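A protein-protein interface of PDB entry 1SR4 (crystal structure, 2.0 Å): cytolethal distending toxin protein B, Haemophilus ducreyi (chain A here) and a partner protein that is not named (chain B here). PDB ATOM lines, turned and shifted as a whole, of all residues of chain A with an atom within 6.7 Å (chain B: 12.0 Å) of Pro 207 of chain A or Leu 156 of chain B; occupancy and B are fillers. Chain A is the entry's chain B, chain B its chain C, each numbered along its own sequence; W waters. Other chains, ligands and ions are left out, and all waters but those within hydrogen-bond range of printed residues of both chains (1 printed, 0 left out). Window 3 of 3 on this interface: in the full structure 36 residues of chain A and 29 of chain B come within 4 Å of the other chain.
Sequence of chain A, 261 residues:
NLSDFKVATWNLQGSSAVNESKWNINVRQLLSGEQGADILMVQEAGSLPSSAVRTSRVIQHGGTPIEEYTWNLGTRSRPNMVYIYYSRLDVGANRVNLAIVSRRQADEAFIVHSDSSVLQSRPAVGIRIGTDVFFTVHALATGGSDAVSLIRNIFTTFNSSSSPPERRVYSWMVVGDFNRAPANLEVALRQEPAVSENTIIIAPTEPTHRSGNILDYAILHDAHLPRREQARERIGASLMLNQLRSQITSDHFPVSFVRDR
The backbone NH (N) of Arg 210 of chain A lies within hydrogen-bond range of the backbone carbonyl oxygen (O) of Asp 251 of chain A (2.9 Å). The backbone NH (N) of Phe 253 of chain A lies within hydrogen-bond range of the backbone carbonyl oxygen (O) of Thr 208 of chain A, at 2.8 Å. ND1 of His 209 of chain A sits at hydrogen-bond distance from OG of Ser 211 of chain A, at 2.8 Å.
Of chain A, only Pro 207, His 209, Arg 210 and Phe 253 come within 4 Å of Leu 156 of chain B. No residue of chain B comes within 4 Å of Pro 204 of chain A. Arg 210 of chain A touches just one residue of chain B: Leu 156. No residue of chain B comes within 4 Å of Ser 211 of chain A. Of chain B, only Ile 157 and Pro 158 come within 4 Å of Gly 212 of chain A. No residue of chain B comes within 4 Å of Ile 214 of chain A. Of chain B, only Leu 156 comes within 4 Å of Phe 253 of chain A. Of the printed residues of chain A, Ile 157 of chain B touches Gly 212. Printed residues of chain B within 4 Å of His 209 of chain A: Leu 156. Of the printed residues of chain B, Thr 205 of chain A touches Pro 158 (3.98 Å). Of the printed residues of chain A, Pro 158 of chain B touches Thr 205, Pro 207 and Gly 212. Asn 213 of chain A touches none of the printed residues of chain B. The nearest residue of chain B that does not touch Pro 207 of chain A is Ile 157 of chain B (4.1 Å).
Among the printed residues, merely in contact across the chains: Thr 205 of chain A with Pro 158 of chain B, Pro 207 of chain A with Leu 156 of chain B, Pro 207 of chain A with Pro 158 of chain B, His 209 of chain A with Leu 156 of chain B, Arg 210 of chain A with Leu 156 of chain B, Gly 212 of chain A with Ile 157 of chain B, Gly 212 of chain A with Pro 158 of chain B and Phe 253 of chain A with Leu 156 of chain B.
Hydrophobic or aromatic side chains of chain A that line the printed part of chain B: Pro 207 and Phe 253. Hydrophobic or aromatic side chains of chain B within 4 Å of the printed part of chain A: Leu 156 and Pro 158. Among the printed residues, 8 pairs touch across the chains. Among the printed residues, no Asp or Glu carboxylate lies within 4 Å of a Lys or Arg side-chain nitrogen of the other chain.
Water W1 lies within hydrogen-bond range of the backbone carbonyl oxygen (O) of Arg 210 of chain A and the side-chain amino group (NZ) of Lys 154 of chain B.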
ATOM      1  N   PRO A 204       4.187  32.496  12.799  1.00  0.00           N
ATOM      2  CA  PRO A 204       5.569  32.459  13.305  1.00  0.00           C
ATOM      3  C   PRO A 204       6.212  31.199  12.740  1.00  0.00           C
ATOM      4  O   PRO A 204       5.521  30.350  12.191  1.00  0.00           O
ATOM      5  CB  PRO A 204       5.411  32.290  14.818  1.00  0.00           C
ATOM      6  CG  PRO A 204       3.934  32.539  15.105  1.00  0.00           C
ATOM      7  CD  PRO A 204       3.209  32.149  13.848  1.00  0.00           C
ATOM      8  N   THR A 205       7.530  31.085  12.872  1.00  0.00           N
ATOM      9  CA  THR A 205       8.240  29.876  12.460  1.00  0.00           C
ATOM     10  C   THR A 205       8.708  29.227  13.768  1.00  0.00           C
ATOM     11  O   THR A 205       9.387  28.202  13.760  1.00  0.00           O
ATOM     12  CB  THR A 205       9.488  30.165  11.594  1.00  0.00           C
ATOM     13  OG1 THR A 205      10.343  31.079  12.286  1.00  0.00           O
ATOM     14  CG2 THR A 205       9.085  30.735  10.234  1.00  0.00           C
ATOM     15  N   GLU A 206       8.377  29.864  14.892  1.00  0.00           N
ATOM     16  CA  GLU A 206       8.708  29.320  16.201  1.00  0.00           C
ATOM     17  C   GLU A 206       7.437  28.668  16.754  1.00  0.00           C
ATOM     18  O   GLU A 206       6.337  29.088  16.446  1.00  0.00           O
ATOM     19  CB  GLU A 206       9.134  30.415  17.175  1.00  0.00           C
ATOM     20  CG  GLU A 206      10.439  31.118  16.851  1.00  0.00           C
ATOM     21  CD  GLU A 206      10.892  31.977  18.009  1.00  0.00           C
ATOM     22  OE1 GLU A 206      10.531  33.172  18.062  1.00  0.00           O
ATOM     23  OE2 GLU A 206      11.596  31.440  18.893  1.00  0.00           O
ATOM     24  N   PRO A 207       7.588  27.641  17.592  1.00  0.00           N
ATOM     25  CA  PRO A 207       6.447  26.938  18.190  1.00  0.00           C
ATOM     26  C   PRO A 207       5.489  27.904  18.920  1.00  0.00           C
ATOM     27  O   PRO A 207       5.932  28.907  19.491  1.00  0.00           O
ATOM     28  CB  PRO A 207       7.121  25.966  19.162  1.00  0.00           C
ATOM     29  CG  PRO A 207       8.436  25.654  18.475  1.00  0.00           C
ATOM     30  CD  PRO A 207       8.872  27.015  17.967  1.00  0.00           C
ATOM     31  N   THR A 208       4.184  27.635  18.861  1.00  0.00           N
ATOM     32  CA  THR A 208       3.213  28.482  19.583  1.00  0.00           C
ATOM     33  C   THR A 208       2.508  27.639  20.638  1.00  0.00           C
ATOM     34  O   THR A 208       1.577  28.104  21.297  1.00  0.00           O
ATOM     35  CB  THR A 208       2.111  29.089  18.676  1.00  0.00           C
ATOM     36  OG1 THR A 208       1.226  28.050  18.230  1.00  0.00           O
ATOM     37  CG2 THR A 208       2.726  29.790  17.467  1.00  0.00           C
ATOM     38  N   HIS A 209       2.966  26.399  20.805  1.00  0.00           N
ATOM     39  CA  HIS A 209       2.373  25.466  21.777  1.00  0.00           C
ATOM     40  C   HIS A 209       3.503  24.609  22.331  1.00  0.00           C
ATOM     41  O   HIS A 209       4.505  24.388  21.653  1.00  0.00           O
ATOM     42  CB  HIS A 209       1.320  24.607  21.077  1.00  0.00           C
ATOM     43  CG  HIS A 209       0.626  23.632  21.977  1.00  0.00           C
ATOM     44  ND1 HIS A 209       0.788  22.269  21.857  1.00  0.00           N
ATOM     45  CD2 HIS A 209      -0.263  23.818  22.983  1.00  0.00           C
ATOM     46  CE1 HIS A 209       0.032  21.656  22.751  1.00  0.00           C
ATOM     47  NE2 HIS A 209      -0.615  22.573  23.449  1.00  0.00           N
ATOM     48  N   ARG A 210       3.351  24.120  23.559  1.00  0.00           N
ATOM     49  CA  ARG A 210       4.417  23.365  24.167  1.00  0.00           C
ATOM     50  C   ARG A 210       4.691  21.999  23.573  1.00  0.00           C
ATOM     51  O   ARG A 210       5.608  21.302  23.995  1.00  0.00           O
ATOM     52  CB  ARG A 210       4.206  23.312  25.689  1.00  0.00           C
ATOM     53  CG  ARG A 210       4.415  24.711  26.316  1.00  0.00           C
ATOM     54  CD  ARG A 210       4.364  24.739  27.851  1.00  0.00           C
ATOM     55  NE  ARG A 210       4.225  26.111  28.350  1.00  0.00           N
ATOM     56  CZ  ARG A 210       4.467  26.489  29.603  1.00  0.00           C
ATOM     57  NH1 ARG A 210       4.871  25.592  30.503  1.00  0.00           N
ATOM     58  NH2 ARG A 210       4.297  27.765  29.959  1.00  0.00           N
ATOM     59  N   SER A 211       3.915  21.626  22.569  1.00  0.00           N
ATOM     60  CA  SER A 211       4.129  20.354  21.892  1.00  0.00           C
ATOM     61  C   SER A 211       5.245  20.577  20.872  1.00  0.00           C
ATOM     62  O   SER A 211       5.800  19.630  20.321  1.00  0.00           O
ATOM     63  CB  SER A 211       2.865  19.952  21.135  1.00  0.00           C
ATOM     64  OG  SER A 211       2.551  20.965  20.181  1.00  0.00           O
ATOM     65  N   GLY A 212       5.547  21.849  20.616  1.00  0.00           N
ATOM     66  CA  GLY A 212       6.551  22.201  19.630  1.00  0.00           C
ATOM     67  C   GLY A 212       5.866  22.621  18.328  1.00  0.00           C
ATOM     68  O   GLY A 212       6.503  23.177  17.425  1.00  0.00           O
ATOM     69  N   ASN A 213       4.560  22.372  18.225  1.00  0.00           N
ATOM     70  CA  ASN A 213       3.812  22.733  17.008  1.00  0.00           C
ATOM     71  C   ASN A 213       3.466  24.213  16.838  1.00  0.00           C
ATOM     72  O   ASN A 213       3.399  24.969  17.808  1.00  0.00           O
ATOM     73  CB  ASN A 213       2.509  21.927  16.933  1.00  0.00           C
ATOM     74  CG  ASN A 213       2.752  20.443  16.686  1.00  0.00           C
ATOM     75  OD1 ASN A 213       3.481  20.078  15.772  1.00  0.00           O
ATOM     76  ND2 ASN A 213       2.131  19.589  17.489  1.00  0.00           N
ATOM     77  N   ILE A 214       3.255  24.620  15.588  1.00  0.00           N
ATOM     78  CA  ILE A 214       2.855  25.989  15.272  1.00  0.00           C
ATOM     79  C   ILE A 214       1.349  25.860  14.972  1.00  0.00           C
ATOM     80  O   ILE A 214       0.952  25.405  13.891  1.00  0.00           O
ATOM     81  CB  ILE A 214       3.622  26.539  14.036  1.00  0.00           C
ATOM     82  CG1 ILE A 214       5.133  26.551  14.320  1.00  0.00           C
ATOM     83  CG2 ILE A 214       3.166  27.971  13.738  1.00  0.00           C
ATOM     84  CD1 ILE A 214       6.004  26.725  13.085  1.00  0.00           C
ATOM     85  N   LEU A 215       0.520  26.260  15.939  1.00  0.00           N
ATOM     86  CA  LEU A 215      -0.937  26.129  15.823  1.00  0.00           C
ATOM     87  C   LEU A 215      -1.715  27.449  15.829  1.00  0.00           C
ATOM     88  O   LEU A 215      -2.878  27.487  15.425  1.00  0.00           O
ATOM     89  CB  LEU A 215      -1.448  25.276  16.987  1.00  0.00           C
ATOM     90  CG  LEU A 215      -0.764  23.922  17.248  1.00  0.00           C
ATOM     91  CD1 LEU A 215      -1.238  23.361  18.593  1.00  0.00           C
ATOM     92  CD2 LEU A 215      -1.067  22.938  16.092  1.00  0.00           C
ATOM     93  N   LEU A 239       5.957  35.466  18.181  1.00  0.00           N
ATOM     94  CA  LEU A 239       5.478  35.137  19.526  1.00  0.00           C
ATOM     95  C   LEU A 239       5.535  36.515  20.198  1.00  0.00           C
ATOM     96  O   LEU A 239       6.500  37.258  19.997  1.00  0.00           O
ATOM     97  CB  LEU A 239       6.428  34.156  20.233  1.00  0.00           C
ATOM     98  CG  LEU A 239       6.577  32.781  19.560  1.00  0.00           C
ATOM     99  CD1 LEU A 239       7.465  31.871  20.396  1.00  0.00           C
ATOM    100  CD2 LEU A 239       5.183  32.156  19.384  1.00  0.00           C
ATOM    101  N   ASP A 251      -0.603  26.282  27.798  1.00  0.00           N
ATOM    102  CA  ASP A 251       0.411  25.632  26.972  1.00  0.00           C
ATOM    103  C   ASP A 251       0.616  26.329  25.616  1.00  0.00           C
ATOM    104  O   ASP A 251       1.401  25.862  24.803  1.00  0.00           O
ATOM    105  CB  ASP A 251       0.057  24.155  26.747  1.00  0.00           C
ATOM    106  CG  ASP A 251       0.240  23.311  27.998  1.00  0.00           C
ATOM    107  OD1 ASP A 251       0.988  23.728  28.909  1.00  0.00           O
ATOM    108  OD2 ASP A 251      -0.356  22.217  28.057  1.00  0.00           O
ATOM    109  N   PHE A 253       1.530  29.938  23.439  1.00  0.00           N
ATOM    110  CA  PHE A 253       2.256  31.196  23.565  1.00  0.00           C
ATOM    111  C   PHE A 253       1.466  32.249  22.783  1.00  0.00           C
ATOM    112  O   PHE A 253       0.956  31.971  21.697  1.00  0.00           O
ATOM    113  CB  PHE A 253       3.663  31.028  22.981  1.00  0.00           C
ATOM    114  CG  PHE A 253       4.542  30.113  23.797  1.00  0.00           C
ATOM    115  CD1 PHE A 253       5.331  30.623  24.823  1.00  0.00           C
ATOM    116  CD2 PHE A 253       4.528  28.746  23.583  1.00  0.00           C
ATOM    117  CE1 PHE A 253       6.089  29.784  25.628  1.00  0.00           C
ATOM    118  CE2 PHE A 253       5.279  27.893  24.378  1.00  0.00           C
ATOM    119  CZ  PHE A 253       6.066  28.420  25.409  1.00  0.00           C
ATOM    120  N   VAL A 255       0.637  35.211  20.288  1.00  0.00           N
ATOM    121  CA  VAL A 255       1.245  35.560  19.006  1.00  0.00           C
ATOM    122  C   VAL A 255       0.733  36.935  18.580  1.00  0.00           C
ATOM    123  O   VAL A 255      -0.460  37.199  18.694  1.00  0.00           O
ATOM    124  CB  VAL A 255       0.843  34.529  17.939  1.00  0.00           C
ATOM    125  CG1 VAL A 255       1.448  34.915  16.572  1.00  0.00           C
ATOM    126  CG2 VAL A 255       1.321  33.135  18.376  1.00  0.00           C
ATOM    127  N   PRO B 148       8.329  31.341  35.345  1.00  0.00           N
ATOM    128  CA  PRO B 148       8.454  29.942  34.922  1.00  0.00           C
ATOM    129  C   PRO B 148       9.086  29.162  36.090  1.00  0.00           C
ATOM    130  O   PRO B 148       9.865  29.713  36.873  1.00  0.00           O
ATOM    131  CB  PRO B 148       9.373  30.029  33.697  1.00  0.00           C
ATOM    132  CG  PRO B 148       9.029  31.401  33.105  1.00  0.00           C
ATOM    133  CD  PRO B 148       8.952  32.256  34.363  1.00  0.00           C
ATOM    134  N   PRO B 152      15.219  22.322  34.994  1.00  0.00           N
ATOM    135  CA  PRO B 152      15.513  21.998  33.598  1.00  0.00           C
ATOM    136  C   PRO B 152      14.318  22.274  32.716  1.00  0.00           C
ATOM    137  O   PRO B 152      13.193  22.397  33.194  1.00  0.00           O
ATOM    138  CB  PRO B 152      15.849  20.517  33.660  1.00  0.00           C
ATOM    139  CG  PRO B 152      14.922  20.022  34.738  1.00  0.00           C
ATOM    140  CD  PRO B 152      15.047  21.100  35.801  1.00  0.00           C
ATOM    141  N   SER B 153      14.571  22.422  31.426  1.00  0.00           N
ATOM    142  CA  SER B 153      13.513  22.638  30.464  1.00  0.00           C
ATOM    143  C   SER B 153      14.120  22.353  29.096  1.00  0.00           C
ATOM    144  O   SER B 153      15.335  22.379  28.920  1.00  0.00           O
ATOM    145  CB  SER B 153      12.950  24.072  30.539  1.00  0.00           C
ATOM    146  OG  SER B 153      13.847  25.049  30.035  1.00  0.00           O
ATOM    147  N   LYS B 154      13.277  22.072  28.124  1.00  0.00           N
ATOM    148  CA  LYS B 154      13.770  21.766  26.799  1.00  0.00           C
ATOM    149  C   LYS B 154      13.336  22.808  25.788  1.00  0.00           C
ATOM    150  O   LYS B 154      12.181  23.228  25.784  1.00  0.00           O
ATOM    151  CB  LYS B 154      13.259  20.377  26.390  1.00  0.00           C
ATOM    152  CG  LYS B 154      13.316  20.093  24.899  1.00  0.00           C
ATOM    153  CD  LYS B 154      12.711  18.720  24.562  1.00  0.00           C
ATOM    154  CE  LYS B 154      11.241  18.644  24.918  1.00  0.00           C
ATOM    155  NZ  LYS B 154      10.424  19.628  24.149  1.00  0.00           N
ATOM    156  N   ILE B 155      14.274  23.236  24.953  1.00  0.00           N
ATOM    157  CA  ILE B 155      13.982  24.183  23.888  1.00  0.00           C
ATOM    158  C   ILE B 155      12.928  23.525  22.992  1.00  0.00           C
ATOM    159  O   ILE B 155      13.114  22.387  22.549  1.00  0.00           O
ATOM    160  CB  ILE B 155      15.212  24.447  22.991  1.00  0.00           C
ATOM    161  CG1 ILE B 155      16.347  25.070  23.797  1.00  0.00           C
ATOM    162  CG2 ILE B 155      14.820  25.372  21.832  1.00  0.00           C
ATOM    163  CD1 ILE B 155      15.937  26.359  24.424  1.00  0.00           C
ATOM    164  N   LEU B 156      11.839  24.235  22.709  1.00  0.00           N
ATOM    165  CA  LEU B 156      10.792  23.688  21.852  1.00  0.00           C
ATOM    166  C   LEU B 156      11.261  23.674  20.397  1.00  0.00           C
ATOM    167  O   LEU B 156      11.809  24.659  19.904  1.00  0.00           O
ATOM    168  CB  LEU B 156       9.505  24.522  21.977  1.00  0.00           C
ATOM    169  CG  LEU B 156       8.861  24.528  23.366  1.00  0.00           C
ATOM    170  CD1 LEU B 156       7.683  25.492  23.390  1.00  0.00           C
ATOM    171  CD2 LEU B 156       8.428  23.125  23.732  1.00  0.00           C
ATOM    172  N   ILE B 157      11.027  22.558  19.717  1.00  0.00           N
ATOM    173  CA  ILE B 157      11.433  22.399  18.322  1.00  0.00           C
ATOM    174  C   ILE B 157      10.232  22.111  17.433  1.00  0.00           C
ATOM    175  O   ILE B 157       9.500  21.161  17.673  1.00  0.00           O
ATOM    176  CB  ILE B 157      12.426  21.230  18.183  1.00  0.00           C
ATOM    177  CG1 ILE B 157      13.632  21.471  19.094  1.00  0.00           C
ATOM    178  CG2 ILE B 157      12.884  21.094  16.721  1.00  0.00           C
ATOM    179  CD1 ILE B 157      14.591  20.281  19.137  1.00  0.00           C
ATOM    180  N   PRO B 158      10.017  22.933  16.396  1.00  0.00           N
ATOM    181  CA  PRO B 158       8.881  22.716  15.496  1.00  0.00           C
ATOM    182  C   PRO B 158       9.120  21.491  14.609  1.00  0.00           C
ATOM    183  O   PRO B 158      10.300  21.220  14.315  1.00  0.00           O
ATOM    184  CB  PRO B 158       8.823  24.022  14.696  1.00  0.00           C
ATOM    185  CG  PRO B 158      10.281  24.418  14.607  1.00  0.00           C
ATOM    186  CD  PRO B 158      10.796  24.122  16.003  1.00  0.00           C
HETATM  187  O   HOH W   1       7.399  19.459  23.846  1.00  0.00           O
